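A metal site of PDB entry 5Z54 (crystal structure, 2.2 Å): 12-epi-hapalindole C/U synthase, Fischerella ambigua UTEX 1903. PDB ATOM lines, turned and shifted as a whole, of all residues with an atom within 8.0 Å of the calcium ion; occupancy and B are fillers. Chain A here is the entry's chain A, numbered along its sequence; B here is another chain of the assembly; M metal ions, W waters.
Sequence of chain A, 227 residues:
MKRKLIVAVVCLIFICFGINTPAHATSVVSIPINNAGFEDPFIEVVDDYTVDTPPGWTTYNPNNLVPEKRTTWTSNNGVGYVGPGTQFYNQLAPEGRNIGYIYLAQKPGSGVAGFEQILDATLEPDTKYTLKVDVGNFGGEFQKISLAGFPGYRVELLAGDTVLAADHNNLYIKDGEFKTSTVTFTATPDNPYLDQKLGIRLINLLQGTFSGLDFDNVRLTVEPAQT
The backbone carbonyl oxygen of Ala 148 is in hydrogen-bond range of the backbone NH of Phe 210 (2.9 Å). The side-chain amide nitrogen (ND2) of Asn 137 lies within hydrogen-bond range of the backbone carbonyl oxygen (O) of Ile 173 (2.8 Å). O of Asn 137 lies within hydrogen-bond range of N of Gly 176 (2.5 Å). The side-chain hydroxyl (OH) of Tyr 89 sits at hydrogen-bond distance from the backbone NH (N) of Phe 138, 3.3 Å away. N of Asn 137 lies within hydrogen-bond range of O of Glu 177 (3.1 Å). N of Leu 147 sits at hydrogen-bond distance from O of Gly 140, 2.9 Å away. N of Ala 148 is in hydrogen-bond range of OG of Ser 146, at 3.3 Å.
Residues that only touch the calcium ion: Ala 148. Six residues have an atom within 4 Å of the calcium ion: Asn 137, Phe 138, Leu 147, Ala 148, Gly 149 and Asp 175. The nearest printed residue that does not touch the calcium ion is Gly 139 (4.3 Å).
The calcium ion is bound by O of Phe 138 (2.3 Å), O of Gly 149 (2.3 Å), OD1 of Asn 137 (2.3 Å), O of Leu 147 (2.3 Å), OD1 of Asp 175 (2.3 Å) and water W1 (2.4 Å). The calcium ion has six donor atoms within binding distance.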
ATOM      1  N   PHE A  88     -24.939  30.488  -4.686  1.00  0.00           N
ATOM      2  CA  PHE A  88     -24.288  29.971  -3.472  1.00  0.00           C
ATOM      3  C   PHE A  88     -23.613  28.641  -3.708  1.00  0.00           C
ATOM      4  O   PHE A  88     -22.758  28.233  -2.926  1.00  0.00           O
ATOM      5  CB  PHE A  88     -25.308  29.669  -2.375  1.00  0.00           C
ATOM      6  CG  PHE A  88     -26.013  30.891  -1.845  1.00  0.00           C
ATOM      7  CD1 PHE A  88     -25.309  32.057  -1.592  1.00  0.00           C
ATOM      8  CD2 PHE A  88     -27.383  30.869  -1.607  1.00  0.00           C
ATOM      9  CE1 PHE A  88     -25.955  33.181  -1.093  1.00  0.00           C
ATOM     10  CE2 PHE A  88     -28.033  31.998  -1.117  1.00  0.00           C
ATOM     11  CZ  PHE A  88     -27.308  33.159  -0.873  1.00  0.00           C
ATOM     12  N   TYR A  89     -24.045  27.931  -4.738  1.00  0.00           N
ATOM     13  CA  TYR A  89     -23.601  26.578  -4.884  1.00  0.00           C
ATOM     14  C   TYR A  89     -23.224  26.334  -6.323  1.00  0.00           C
ATOM     15  O   TYR A  89     -23.720  27.022  -7.208  1.00  0.00           O
ATOM     16  CB  TYR A  89     -24.675  25.633  -4.335  1.00  0.00           C
ATOM     17  CG  TYR A  89     -24.644  25.546  -2.841  1.00  0.00           C
ATOM     18  CD1 TYR A  89     -23.555  24.963  -2.196  1.00  0.00           C
ATOM     19  CD2 TYR A  89     -25.642  26.090  -2.070  1.00  0.00           C
ATOM     20  CE1 TYR A  89     -23.478  24.887  -0.816  1.00  0.00           C
ATOM     21  CE2 TYR A  89     -25.580  26.042  -0.683  1.00  0.00           C
ATOM     22  CZ  TYR A  89     -24.505  25.435  -0.068  1.00  0.00           C
ATOM     23  OH  TYR A  89     -24.420  25.368   1.290  1.00  0.00           O
ATOM     24  N   GLY A 136     -23.108  21.563   3.918  1.00  0.00           N
ATOM     25  CA  GLY A 136     -22.864  22.475   2.822  1.00  0.00           C
ATOM     26  C   GLY A 136     -22.095  23.726   3.243  1.00  0.00           C
ATOM     27  O   GLY A 136     -22.374  24.336   4.290  1.00  0.00           O
ATOM     28  N   ASN A 137     -21.124  24.087   2.397  1.00  0.00           N
ATOM     29  CA  ASN A 137     -20.347  25.296   2.531  1.00  0.00           C
ATOM     30  C   ASN A 137     -20.818  26.271   1.437  1.00  0.00           C
ATOM     31  O   ASN A 137     -20.384  26.170   0.311  1.00  0.00           O
ATOM     32  CB  ASN A 137     -18.862  24.955   2.327  1.00  0.00           C
ATOM     33  CG  ASN A 137     -17.944  26.142   2.530  1.00  0.00           C
ATOM     34  OD1 ASN A 137     -18.392  27.252   2.818  1.00  0.00           O
ATOM     35  ND2 ASN A 137     -16.639  25.912   2.426  1.00  0.00           N
ATOM     36  N   PHE A 138     -21.707  27.208   1.756  1.00  0.00           N
ATOM     37  CA  PHE A 138     -22.113  28.101   0.683  1.00  0.00           C
ATOM     38  C   PHE A 138     -21.018  29.143   0.414  1.00  0.00           C
ATOM     39  O   PHE A 138     -20.327  29.596   1.318  1.00  0.00           O
ATOM     40  CB  PHE A 138     -23.536  28.629   0.827  1.00  0.00           C
ATOM     41  CG  PHE A 138     -23.840  29.423   2.072  1.00  0.00           C
ATOM     42  CD1 PHE A 138     -24.283  28.776   3.220  1.00  0.00           C
ATOM     43  CD2 PHE A 138     -23.740  30.805   2.063  1.00  0.00           C
ATOM     44  CE1 PHE A 138     -24.598  29.510   4.360  1.00  0.00           C
ATOM     45  CE2 PHE A 138     -24.032  31.531   3.202  1.00  0.00           C
ATOM     46  CZ  PHE A 138     -24.452  30.888   4.356  1.00  0.00           C
ATOM     47  N   GLY A 139     -20.853  29.405  -0.868  1.00  0.00           N
ATOM     48  CA  GLY A 139     -19.899  30.404  -1.352  1.00  0.00           C
ATOM     49  C   GLY A 139     -20.662  31.540  -1.985  1.00  0.00           C
ATOM     50  O   GLY A 139     -21.846  31.697  -1.714  1.00  0.00           O
ATOM     51  N   GLY A 140     -19.995  32.308  -2.839  1.00  0.00           N
ATOM     52  CA  GLY A 140     -20.679  33.447  -3.451  1.00  0.00           C
ATOM     53  C   GLY A 140     -20.324  34.719  -2.744  1.00  0.00           C
ATOM     54  O   GLY A 140     -19.569  34.674  -1.794  1.00  0.00           O
ATOM     55  N   SER A 146     -18.229  38.681   1.422  1.00  0.00           N
ATOM     56  CA  SER A 146     -17.811  37.420   0.785  1.00  0.00           C
ATOM     57  C   SER A 146     -18.357  36.250   1.607  1.00  0.00           C
ATOM     58  O   SER A 146     -18.387  36.376   2.806  1.00  0.00           O
ATOM     59  CB  SER A 146     -16.333  37.356   0.690  1.00  0.00           C
ATOM     60  OG  SER A 146     -15.933  36.173   0.038  1.00  0.00           O
ATOM     61  N   LEU A 147     -18.747  35.161   0.962  1.00  0.00           N
ATOM     62  CA  LEU A 147     -19.238  33.974   1.712  1.00  0.00           C
ATOM     63  C   LEU A 147     -18.136  32.921   1.729  1.00  0.00           C
ATOM     64  O   LEU A 147     -18.356  31.833   2.251  1.00  0.00           O
ATOM     65  CB  LEU A 147     -20.541  33.502   1.083  1.00  0.00           C
ATOM     66  CG  LEU A 147     -21.599  34.591   0.999  1.00  0.00           C
ATOM     67  CD1 LEU A 147     -22.920  34.047   0.515  1.00  0.00           C
ATOM     68  CD2 LEU A 147     -21.764  35.277   2.332  1.00  0.00           C
ATOM     69  N   ALA A 148     -16.973  33.277   1.186  1.00  0.00           N
ATOM     70  CA  ALA A 148     -15.812  32.392   1.204  1.00  0.00           C
ATOM     71  C   ALA A 148     -15.464  32.063   2.652  1.00  0.00           C
ATOM     72  O   ALA A 148     -15.619  32.899   3.533  1.00  0.00           O
ATOM     73  CB  ALA A 148     -14.650  33.070   0.500  1.00  0.00           C
ATOM     74  N   GLY A 149     -14.989  30.830   2.875  1.00  0.00           N
ATOM     75  CA  GLY A 149     -14.570  30.402   4.207  1.00  0.00           C
ATOM     76  C   GLY A 149     -15.729  29.631   4.843  1.00  0.00           C
ATOM     77  O   GLY A 149     -16.809  29.585   4.247  1.00  0.00           O
ATOM     78  N   PHE A 150     -15.502  29.059   6.034  1.00  0.00           N
ATOM     79  CA  PHE A 150     -16.382  28.060   6.597  1.00  0.00           C
ATOM     80  C   PHE A 150     -16.234  28.038   8.106  1.00  0.00           C
ATOM     81  O   PHE A 150     -15.136  28.148   8.611  1.00  0.00           O
ATOM     82  CB  PHE A 150     -16.025  26.695   6.024  1.00  0.00           C
ATOM     83  CG  PHE A 150     -16.957  25.563   6.370  1.00  0.00           C
ATOM     84  CD1 PHE A 150     -18.290  25.591   5.962  1.00  0.00           C
ATOM     85  CD2 PHE A 150     -16.497  24.441   7.053  1.00  0.00           C
ATOM     86  CE1 PHE A 150     -19.147  24.522   6.232  1.00  0.00           C
ATOM     87  CE2 PHE A 150     -17.357  23.386   7.342  1.00  0.00           C
ATOM     88  CZ  PHE A 150     -18.686  23.426   6.926  1.00  0.00           C
ATOM     89  N   PRO A 151     -17.358  27.942   8.862  1.00  0.00           N
ATOM     90  CA  PRO A 151     -17.279  27.938  10.321  1.00  0.00           C
ATOM     91  C   PRO A 151     -16.840  26.637  11.007  1.00  0.00           C
ATOM     92  O   PRO A 151     -16.450  26.673  12.175  1.00  0.00           O
ATOM     93  CB  PRO A 151     -18.708  28.341  10.708  1.00  0.00           C
ATOM     94  CG  PRO A 151     -19.547  27.722   9.603  1.00  0.00           C
ATOM     95  CD  PRO A 151     -18.735  27.997   8.365  1.00  0.00           C
ATOM     96  N   ILE A 173     -14.686  20.734   3.149  1.00  0.00           N
ATOM     97  CA  ILE A 173     -15.770  21.106   2.230  1.00  0.00           C
ATOM     98  C   ILE A 173     -15.457  22.465   1.632  1.00  0.00           C
ATOM     99  O   ILE A 173     -15.382  23.447   2.355  1.00  0.00           O
ATOM    100  CB  ILE A 173     -17.112  21.160   2.967  1.00  0.00           C
ATOM    101  CG1 ILE A 173     -17.342  19.899   3.803  1.00  0.00           C
ATOM    102  CG2 ILE A 173     -18.246  21.435   1.975  1.00  0.00           C
ATOM    103  CD1 ILE A 173     -18.581  19.936   4.636  1.00  0.00           C
ATOM    104  N   LYS A 174     -15.323  22.521   0.310  1.00  0.00           N
ATOM    105  CA  LYS A 174     -14.961  23.733  -0.396  1.00  0.00           C
ATOM    106  C   LYS A 174     -16.178  24.648  -0.544  1.00  0.00           C
ATOM    107  O   LYS A 174     -17.292  24.143  -0.535  1.00  0.00           O
ATOM    108  CB  LYS A 174     -14.418  23.340  -1.764  1.00  0.00           C
ATOM    109  CG  LYS A 174     -12.907  23.269  -1.827  1.00  0.00           C
ATOM    110  CD  LYS A 174     -12.337  22.450  -2.976  1.00  0.00           C
ATOM    111  CE  LYS A 174     -10.836  22.607  -3.079  1.00  0.00           C
ATOM    112  NZ  LYS A 174     -10.142  21.298  -2.988  1.00  0.00           N
ATOM    113  N   ASP A 175     -15.967  25.982  -0.716  1.00  0.00           N
ATOM    114  CA  ASP A 175     -17.066  26.918  -0.939  1.00  0.00           C
ATOM    115  C   ASP A 175     -17.926  26.428  -2.104  1.00  0.00           C
ATOM    116  O   ASP A 175     -17.404  26.041  -3.139  1.00  0.00           O
ATOM    117  CB  ASP A 175     -16.587  28.350  -1.201  1.00  0.00           C
ATOM    118  CG  ASP A 175     -16.007  29.056   0.032  1.00  0.00           C
ATOM    119  OD1 ASP A 175     -16.807  29.378   0.979  1.00  0.00           O
ATOM    120  OD2 ASP A 175     -14.767  29.258   0.060  1.00  0.00           O
ATOM    121  N   GLY A 176     -19.236  26.381  -1.920  1.00  0.00           N
ATOM    122  CA  GLY A 176     -20.108  26.055  -3.051  1.00  0.00           C
ATOM    123  C   GLY A 176     -20.366  24.559  -3.238  1.00  0.00           C
ATOM    124  O   GLY A 176     -20.988  24.149  -4.226  1.00  0.00           O
ATOM    125  N   GLU A 177     -19.930  23.736  -2.270  1.00  0.00           N
ATOM    126  CA  GLU A 177     -20.085  22.302  -2.416  1.00  0.00           C
ATOM    127  C   GLU A 177     -20.693  21.692  -1.161  1.00  0.00           C
ATOM    128  O   GLU A 177     -20.746  22.346  -0.111  1.00  0.00           O
ATOM    129  CB  GLU A 177     -18.785  21.677  -2.933  1.00  0.00           C
ATOM    130  CG  GLU A 177     -17.829  21.184  -1.856  1.00  0.00           C
ATOM    131  CD  GLU A 177     -16.591  20.419  -2.349  1.00  0.00           C
ATOM    132  OE1 GLU A 177     -16.411  20.320  -3.608  1.00  0.00           O
ATOM    133  OE2 GLU A 177     -15.789  19.927  -1.497  1.00  0.00           O
ATOM    134  N   THR A 209     -14.750  32.311   9.518  1.00  0.00           N
ATOM    135  CA  THR A 209     -15.668  33.127   8.718  1.00  0.00           C
ATOM    136  C   THR A 209     -15.389  32.857   7.242  1.00  0.00           C
ATOM    137  O   THR A 209     -14.256  32.534   6.898  1.00  0.00           O
ATOM    138  CB  THR A 209     -15.469  34.628   8.985  1.00  0.00           C
ATOM    139  OG1 THR A 209     -14.155  34.975   8.548  1.00  0.00           O
ATOM    140  CG2 THR A 209     -15.664  35.016  10.430  1.00  0.00           C
ATOM    141  N   PHE A 210     -16.386  33.010   6.354  1.00  0.00           N
ATOM    142  CA  PHE A 210     -17.760  33.411   6.653  1.00  0.00           C
ATOM    143  C   PHE A 210     -18.467  32.342   7.507  1.00  0.00           C
ATOM    144  O   PHE A 210     -18.348  31.161   7.238  1.00  0.00           O
ATOM    145  CB  PHE A 210     -18.475  33.623   5.330  1.00  0.00           C
ATOM    146  CG  PHE A 210     -19.903  34.069   5.483  1.00  0.00           C
ATOM    147  CD1 PHE A 210     -20.206  35.389   5.774  1.00  0.00           C
ATOM    148  CD2 PHE A 210     -20.956  33.145   5.401  1.00  0.00           C
ATOM    149  CE1 PHE A 210     -21.516  35.800   5.941  1.00  0.00           C
ATOM    150  CE2 PHE A 210     -22.266  33.556   5.568  1.00  0.00           C
ATOM    151  CZ  PHE A 210     -22.552  34.875   5.842  1.00  0.00           C
ATOM    152  N   SER A 211     -19.309  32.775   8.473  1.00  0.00           N
ATOM    153  CA  SER A 211     -19.820  31.896   9.524  1.00  0.00           C
ATOM    154  C   SER A 211     -21.234  31.358   9.258  1.00  0.00           C
ATOM    155  O   SER A 211     -22.069  31.305  10.180  1.00  0.00           O
ATOM    156  CB  SER A 211     -19.751  32.602  10.857  1.00  0.00           C
ATOM    157  OG  SER A 211     -18.395  32.905  11.182  1.00  0.00           O
ATOM    158  N   GLY A 212     -21.503  30.893   8.047  1.00  0.00           N
ATOM    159  CA  GLY A 212     -22.732  30.151   7.820  1.00  0.00           C
ATOM    160  C   GLY A 212     -22.434  28.793   7.201  1.00  0.00           C
ATOM    161  O   GLY A 212     -21.444  28.617   6.513  1.00  0.00           O
ATOM    162  N   LEU A 213     -23.317  27.827   7.435  1.00  0.00           N
ATOM    163  CA  LEU A 213     -23.224  26.562   6.720  1.00  0.00           C
ATOM    164  C   LEU A 213     -24.637  25.987   6.622  1.00  0.00           C
ATOM    165  O   LEU A 213     -25.553  26.495   7.257  1.00  0.00           O
ATOM    166  CB  LEU A 213     -22.292  25.633   7.510  1.00  0.00           C
ATOM    167  CG  LEU A 213     -22.876  24.825   8.686  1.00  0.00           C
ATOM    168  CD1 LEU A 213     -21.841  23.829   9.202  1.00  0.00           C
ATOM    169  CD2 LEU A 213     -23.290  25.732   9.814  1.00  0.00           C
ATOM    170  N   ASP B 190      -7.425  31.330   5.331  1.00  0.00           N
ATOM    171  CA  ASP B 190      -8.456  32.072   6.044  1.00  0.00           C
ATOM    172  C   ASP B 190      -8.426  31.756   7.546  1.00  0.00           C
ATOM    173  O   ASP B 190      -8.896  32.546   8.372  1.00  0.00           O
ATOM    174  CB  ASP B 190      -9.846  31.670   5.546  1.00  0.00           C
ATOM    175  CG  ASP B 190     -10.308  32.440   4.319  1.00  0.00           C
ATOM    176  OD1 ASP B 190      -9.473  33.186   3.755  1.00  0.00           O
ATOM    177  OD2 ASP B 190     -11.506  32.298   3.947  1.00  0.00           O
HETATM  178 CA    CA M   1     -18.446  29.552   2.632  1.00  0.00          CA
HETATM  179  O   HOH W   1     -20.067  29.552   4.393  1.00  0.00           O
